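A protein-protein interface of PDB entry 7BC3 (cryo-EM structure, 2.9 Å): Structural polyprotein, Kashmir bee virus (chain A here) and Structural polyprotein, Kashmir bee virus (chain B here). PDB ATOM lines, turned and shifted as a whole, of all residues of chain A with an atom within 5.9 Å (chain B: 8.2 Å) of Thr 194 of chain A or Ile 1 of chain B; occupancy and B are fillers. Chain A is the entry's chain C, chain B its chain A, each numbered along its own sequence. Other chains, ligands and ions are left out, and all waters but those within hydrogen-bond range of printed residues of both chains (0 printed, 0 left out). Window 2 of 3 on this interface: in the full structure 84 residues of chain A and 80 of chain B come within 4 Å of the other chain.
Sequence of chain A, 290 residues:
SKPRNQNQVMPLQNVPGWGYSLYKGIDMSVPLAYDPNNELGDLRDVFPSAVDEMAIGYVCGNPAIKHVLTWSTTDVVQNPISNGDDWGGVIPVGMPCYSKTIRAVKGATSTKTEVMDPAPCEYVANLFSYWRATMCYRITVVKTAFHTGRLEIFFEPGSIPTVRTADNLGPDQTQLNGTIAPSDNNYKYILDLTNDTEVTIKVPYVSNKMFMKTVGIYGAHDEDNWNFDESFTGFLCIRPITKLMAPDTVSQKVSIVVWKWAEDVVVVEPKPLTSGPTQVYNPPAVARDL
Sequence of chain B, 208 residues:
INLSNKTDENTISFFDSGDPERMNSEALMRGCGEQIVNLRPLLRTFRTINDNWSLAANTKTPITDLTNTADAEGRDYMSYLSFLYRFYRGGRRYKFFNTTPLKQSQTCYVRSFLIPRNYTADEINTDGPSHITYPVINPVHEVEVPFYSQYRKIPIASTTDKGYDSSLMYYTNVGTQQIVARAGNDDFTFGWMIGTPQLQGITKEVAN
The backbone carbonyl oxygen (O) of Asn 2 of chain B is in hydrogen-bond range of the side-chain amide nitrogen (ND2) of Asn 195 of chain A (2.6 Å).
The side-chain amide nitrogen of Asn 195 of chain A lies within hydrogen-bond range of the side-chain hydroxyl of Ser 4 of chain B (2.8 Å).
The side-chain amino group of Lys 143 of chain A sits at hydrogen-bond distance from the side-chain amide oxygen of Asn 5 of chain B (2.8 Å).
OD1 of Asn 5 of chain B sits close to O of Thr 144 of chain A (3.3 Å).
O of Asn 195 of chain A sits at hydrogen-bond distance from N of Lys 6 of chain B, at 2.7 Å.
OD1 of Asp 196 of chain A sits close to O of Lys 6 of chain B (3.3 Å).
NZ of Lys 143 of chain A lies within hydrogen-bond range of O of His 147 of chain A (3.3 Å).
The side-chain amino group (NZ) of Lys 143 of chain A is in hydrogen-bond range of the backbone carbonyl oxygen (O) of Leu 193 of chain A.
OG1 of Thr 144 of chain A is in hydrogen-bond range of N of Phe 146 of chain A.
ND1 of His 147 of chain A is in hydrogen-bond range of OG1 of Thr 144 of chain A, 3.0 Å away.
The side-chain carboxylate (OD1) of Asp 192 of chain A sits at hydrogen-bond distance from the side-chain hydroxyl (OG1) of Thr 194 of chain A, 2.7 Å away.
Ala 145 of chain A touches Ser 4 of chain B.
Ala 145 of chain A touches Asn 5 of chain B (CB to N, 3.9 Å).
Thr 194 of chain A touches Ile 1 of chain B (CG2 to CG2, 3.6 Å).
Ser 4 of chain B touches Thr 194 of chain A (O to O, 3.5 Å).
Asn 195 of chain A touches Asn 5 of chain B.
Thr 194 of chain A touches just these residues of chain B: Ile 1 (3.6 Å) and Ser 4 (3.5 Å).
Of chain A, only Thr 194 comes within 4 Å of Ile 1 of chain B.
Printed residues of chain B within 4 Å of Asp 196 of chain A: Lys 6 (3.3 Å).
Of the printed residues of chain A, Asn 5 of chain B touches Lys 143 (2.8 Å), Thr 144 (3.3 Å), Ala 145 (3.9 Å) and Asn 195 (3.4 Å).
Of the printed residues of chain B, Ala 145 of chain A touches Ser 4 (3.6 Å) and Asn 5 (3.9 Å).
Of the printed residues of chain A, Ser 4 of chain B touches Ala 145, Thr 194 and Asn 195.
Of the printed residues of chain B, Asn 195 of chain A touches Asn 2 (2.6 Å), Ser 4 (2.8 Å), Asn 5 (3.4 Å) and Lys 6 (2.7 Å).
His 147 of chain A touches none of the printed residues of chain B.
Gly 149 of chain A touches none of the printed residues of chain B.
The nearest printed residue of chain B that does not touch Thr 194 of chain A is Asn 5 of chain B (5.4 Å).
Of the 12 printed residues of chain A, 6 touch a printed residue of chain B.
Hydrophobic or aromatic side chains of chain A within 4 Å of the printed part of chain B: Ala 145.
Along chain A the printed residues that touch a printed residue of chain B span positions 143 to 196.
Of the 6 printed residues of chain B, 5 touch a printed residue of chain A.
Hydrophobic or aromatic side chains of chain B that line the printed part of chain A: Ile 1.
Among the printed residues, 11 pairs touch across the chains.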
ATOM      1  N   LYS A 143     -13.666 -23.292  23.933  1.00  0.00           N
ATOM      2  CA  LYS A 143     -12.512 -22.742  24.621  1.00  0.00           C
ATOM      3  C   LYS A 143     -12.869 -21.357  25.145  1.00  0.00           C
ATOM      4  O   LYS A 143     -14.041 -20.974  25.197  1.00  0.00           O
ATOM      5  CB  LYS A 143     -11.307 -22.695  23.676  1.00  0.00           C
ATOM      6  CG  LYS A 143     -11.525 -21.789  22.486  1.00  0.00           C
ATOM      7  CD  LYS A 143     -10.273 -21.608  21.673  1.00  0.00           C
ATOM      8  CE  LYS A 143     -10.369 -20.351  20.844  1.00  0.00           C
ATOM      9  NZ  LYS A 143      -9.836 -19.160  21.553  1.00  0.00           N
ATOM     10  N   THR A 144     -11.846 -20.607  25.531  1.00  0.00           N
ATOM     11  CA  THR A 144     -11.962 -19.216  25.936  1.00  0.00           C
ATOM     12  C   THR A 144     -11.083 -18.361  25.031  1.00  0.00           C
ATOM     13  O   THR A 144     -10.502 -18.839  24.055  1.00  0.00           O
ATOM     14  CB  THR A 144     -11.559 -19.028  27.402  1.00  0.00           C
ATOM     15  OG1 THR A 144     -10.141 -19.184  27.534  1.00  0.00           O
ATOM     16  CG2 THR A 144     -12.253 -20.032  28.291  1.00  0.00           C
ATOM     17  N   ALA A 145     -10.989 -17.079  25.367  1.00  0.00           N
ATOM     18  CA  ALA A 145     -10.093 -16.169  24.670  1.00  0.00           C
ATOM     19  C   ALA A 145      -8.649 -16.305  25.125  1.00  0.00           C
ATOM     20  O   ALA A 145      -7.783 -15.596  24.605  1.00  0.00           O
ATOM     21  CB  ALA A 145     -10.560 -14.728  24.863  1.00  0.00           C
ATOM     22  N   PHE A 146      -8.371 -17.195  26.076  1.00  0.00           N
ATOM     23  CA  PHE A 146      -7.036 -17.377  26.622  1.00  0.00           C
ATOM     24  C   PHE A 146      -6.434 -18.729  26.270  1.00  0.00           C
ATOM     25  O   PHE A 146      -5.288 -18.998  26.641  1.00  0.00           O
ATOM     26  CB  PHE A 146      -7.075 -17.193  28.139  1.00  0.00           C
ATOM     27  CG  PHE A 146      -7.887 -16.011  28.571  1.00  0.00           C
ATOM     28  CD1 PHE A 146      -7.314 -14.757  28.660  1.00  0.00           C
ATOM     29  CD2 PHE A 146      -9.230 -16.150  28.868  1.00  0.00           C
ATOM     30  CE1 PHE A 146      -8.061 -13.667  29.046  1.00  0.00           C
ATOM     31  CE2 PHE A 146      -9.982 -15.062  29.256  1.00  0.00           C
ATOM     32  CZ  PHE A 146      -9.396 -13.820  29.344  1.00  0.00           C
ATOM     33  N   HIS A 147      -7.177 -19.584  25.575  1.00  0.00           N
ATOM     34  CA  HIS A 147      -6.617 -20.777  24.961  1.00  0.00           C
ATOM     35  C   HIS A 147      -6.117 -20.422  23.568  1.00  0.00           C
ATOM     36  O   HIS A 147      -6.816 -19.747  22.806  1.00  0.00           O
ATOM     37  CB  HIS A 147      -7.660 -21.889  24.862  1.00  0.00           C
ATOM     38  CG  HIS A 147      -8.130 -22.409  26.183  1.00  0.00           C
ATOM     39  ND1 HIS A 147      -9.301 -21.989  26.773  1.00  0.00           N
ATOM     40  CD2 HIS A 147      -7.599 -23.333  27.016  1.00  0.00           C
ATOM     41  CE1 HIS A 147      -9.466 -22.623  27.919  1.00  0.00           C
ATOM     42  NE2 HIS A 147      -8.446 -23.444  28.091  1.00  0.00           N
ATOM     43  N   THR A 148      -4.912 -20.877  23.238  1.00  0.00           N
ATOM     44  CA  THR A 148      -4.376 -20.714  21.897  1.00  0.00           C
ATOM     45  C   THR A 148      -3.767 -22.032  21.450  1.00  0.00           C
ATOM     46  O   THR A 148      -3.370 -22.868  22.264  1.00  0.00           O
ATOM     47  CB  THR A 148      -3.327 -19.596  21.814  1.00  0.00           C
ATOM     48  OG1 THR A 148      -2.153 -19.976  22.537  1.00  0.00           O
ATOM     49  CG2 THR A 148      -3.870 -18.304  22.389  1.00  0.00           C
ATOM     50  N   GLY A 149      -3.704 -22.207  20.139  1.00  0.00           N
ATOM     51  CA  GLY A 149      -3.160 -23.420  19.569  1.00  0.00           C
ATOM     52  C   GLY A 149      -3.384 -23.435  18.078  1.00  0.00           C
ATOM     53  O   GLY A 149      -4.131 -22.625  17.524  1.00  0.00           O
ATOM     54  N   ASP A 192      -5.914 -21.583  13.474  1.00  0.00           N
ATOM     55  CA  ASP A 192      -5.415 -20.888  14.650  1.00  0.00           C
ATOM     56  C   ASP A 192      -6.561 -20.645  15.623  1.00  0.00           C
ATOM     57  O   ASP A 192      -7.636 -20.188  15.225  1.00  0.00           O
ATOM     58  CB  ASP A 192      -4.764 -19.563  14.254  1.00  0.00           C
ATOM     59  CG  ASP A 192      -3.756 -19.082  15.276  1.00  0.00           C
ATOM     60  OD1 ASP A 192      -3.874 -19.467  16.458  1.00  0.00           O
ATOM     61  OD2 ASP A 192      -2.840 -18.326  14.896  1.00  0.00           O
ATOM     62  N   LEU A 193      -6.323 -20.951  16.896  1.00  0.00           N
ATOM     63  CA  LEU A 193      -7.332 -20.839  17.939  1.00  0.00           C
ATOM     64  C   LEU A 193      -7.190 -19.572  18.766  1.00  0.00           C
ATOM     65  O   LEU A 193      -7.879 -19.427  19.780  1.00  0.00           O
ATOM     66  CB  LEU A 193      -7.261 -22.053  18.861  1.00  0.00           C
ATOM     67  CG  LEU A 193      -8.242 -23.184  18.593  1.00  0.00           C
ATOM     68  CD1 LEU A 193      -8.206 -23.592  17.141  1.00  0.00           C
ATOM     69  CD2 LEU A 193      -7.884 -24.338  19.488  1.00  0.00           C
ATOM     70  N   THR A 194      -6.303 -18.661  18.373  1.00  0.00           N
ATOM     71  CA  THR A 194      -6.098 -17.447  19.154  1.00  0.00           C
ATOM     72  C   THR A 194      -7.421 -16.746  19.432  1.00  0.00           C
ATOM     73  O   THR A 194      -7.748 -16.439  20.583  1.00  0.00           O
ATOM     74  CB  THR A 194      -5.143 -16.515  18.417  1.00  0.00           C
ATOM     75  OG1 THR A 194      -3.994 -17.251  17.979  1.00  0.00           O
ATOM     76  CG2 THR A 194      -4.704 -15.377  19.311  1.00  0.00           C
ATOM     77  N   ASN A 195      -8.189 -16.487  18.388  1.00  0.00           N
ATOM     78  CA  ASN A 195      -9.501 -15.864  18.514  1.00  0.00           C
ATOM     79  C   ASN A 195     -10.606 -16.685  17.871  1.00  0.00           C
ATOM     80  O   ASN A 195     -11.714 -16.741  18.409  1.00  0.00           O
ATOM     81  CB  ASN A 195      -9.477 -14.463  17.894  1.00  0.00           C
ATOM     82  CG  ASN A 195      -8.586 -13.505  18.655  1.00  0.00           C
ATOM     83  OD1 ASN A 195      -7.813 -13.910  19.521  1.00  0.00           O
ATOM     84  ND2 ASN A 195      -8.689 -12.226  18.331  1.00  0.00           N
ATOM     85  N   ASP A 196     -10.336 -17.322  16.738  1.00  0.00           N
ATOM     86  CA  ASP A 196     -11.356 -18.095  16.052  1.00  0.00           C
ATOM     87  C   ASP A 196     -11.566 -19.438  16.750  1.00  0.00           C
ATOM     88  O   ASP A 196     -10.750 -19.893  17.556  1.00  0.00           O
ATOM     89  CB  ASP A 196     -10.968 -18.308  14.589  1.00  0.00           C
ATOM     90  CG  ASP A 196     -12.154 -18.663  13.714  1.00  0.00           C
ATOM     91  OD1 ASP A 196     -13.297 -18.641  14.215  1.00  0.00           O
ATOM     92  OD2 ASP A 196     -11.943 -18.964  12.521  1.00  0.00           O
ATOM     93  N   ILE B   1      -2.380  -8.612  18.679  1.00  0.00           N
ATOM     94  CA  ILE B   1      -3.495  -9.580  18.861  1.00  0.00           C
ATOM     95  C   ILE B   1      -4.508  -9.010  19.843  1.00  0.00           C
ATOM     96  O   ILE B   1      -4.141  -8.334  20.802  1.00  0.00           O
ATOM     97  CB  ILE B   1      -2.973 -10.945  19.336  1.00  0.00           C
ATOM     98  CG1 ILE B   1      -2.140 -11.603  18.236  1.00  0.00           C
ATOM     99  CG2 ILE B   1      -4.124 -11.850  19.728  1.00  0.00           C
ATOM    100  CD1 ILE B   1      -1.196 -12.671  18.741  1.00  0.00           C
ATOM    101  N   ASN B   2      -5.783  -9.299  19.603  1.00  0.00           N
ATOM    102  CA  ASN B   2      -6.879  -8.826  20.437  1.00  0.00           C
ATOM    103  C   ASN B   2      -7.529 -10.006  21.144  1.00  0.00           C
ATOM    104  O   ASN B   2      -7.849 -11.015  20.509  1.00  0.00           O
ATOM    105  CB  ASN B   2      -7.916  -8.078  19.599  1.00  0.00           C
ATOM    106  CG  ASN B   2      -9.208  -7.843  20.346  1.00  0.00           C
ATOM    107  OD1 ASN B   2      -9.232  -7.163  21.372  1.00  0.00           O
ATOM    108  ND2 ASN B   2     -10.293  -8.408  19.836  1.00  0.00           N
ATOM    109  N   LEU B   3      -7.715  -9.880  22.453  1.00  0.00           N
ATOM    110  CA  LEU B   3      -8.364 -10.926  23.230  1.00  0.00           C
ATOM    111  C   LEU B   3      -9.815 -11.070  22.792  1.00  0.00           C
ATOM    112  O   LEU B   3     -10.604 -10.128  22.912  1.00  0.00           O
ATOM    113  CB  LEU B   3      -8.291 -10.604  24.718  1.00  0.00           C
ATOM    114  CG  LEU B   3      -6.896 -10.584  25.332  1.00  0.00           C
ATOM    115  CD1 LEU B   3      -6.964 -10.109  26.768  1.00  0.00           C
ATOM    116  CD2 LEU B   3      -6.253 -11.952  25.248  1.00  0.00           C
ATOM    117  N   SER B   4     -10.167 -12.253  22.294  1.00  0.00           N
ATOM    118  CA  SER B   4     -11.529 -12.514  21.857  1.00  0.00           C
ATOM    119  C   SER B   4     -11.678 -13.994  21.546  1.00  0.00           C
ATOM    120  O   SER B   4     -10.707 -14.669  21.193  1.00  0.00           O
ATOM    121  CB  SER B   4     -11.887 -11.682  20.622  1.00  0.00           C
ATOM    122  OG  SER B   4     -11.299 -12.227  19.455  1.00  0.00           O
ATOM    123  N   ASN B   5     -12.901 -14.487  21.695  1.00  0.00           N
ATOM    124  CA  ASN B   5     -13.294 -15.816  21.235  1.00  0.00           C
ATOM    125  C   ASN B   5     -14.446 -15.595  20.266  1.00  0.00           C
ATOM    126  O   ASN B   5     -15.567 -15.292  20.688  1.00  0.00           O
ATOM    127  CB  ASN B   5     -13.695 -16.720  22.395  1.00  0.00           C
ATOM    128  CG  ASN B   5     -13.601 -18.185  22.044  1.00  0.00           C
ATOM    129  OD1 ASN B   5     -12.606 -18.632  21.482  1.00  0.00           O
ATOM    130  ND2 ASN B   5     -14.641 -18.942  22.365  1.00  0.00           N
ATOM    131  N   LYS B   6     -14.172 -15.736  18.970  1.00  0.00           N
ATOM    132  CA  LYS B   6     -15.158 -15.387  17.959  1.00  0.00           C
ATOM    133  C   LYS B   6     -15.298 -16.470  16.900  1.00  0.00           C
ATOM    134  O   LYS B   6     -14.722 -17.555  17.021  1.00  0.00           O
ATOM    135  CB  LYS B   6     -14.789 -14.056  17.304  1.00  0.00           C
ATOM    136  CG  LYS B   6     -13.482 -14.074  16.540  1.00  0.00           C
ATOM    137  CD  LYS B   6     -13.286 -12.783  15.775  1.00  0.00           C
ATOM    138  CE  LYS B   6     -12.020 -12.818  14.943  1.00  0.00           C
ATOM    139  NZ  LYS B   6     -11.891 -11.614  14.083  1.00  0.00           N
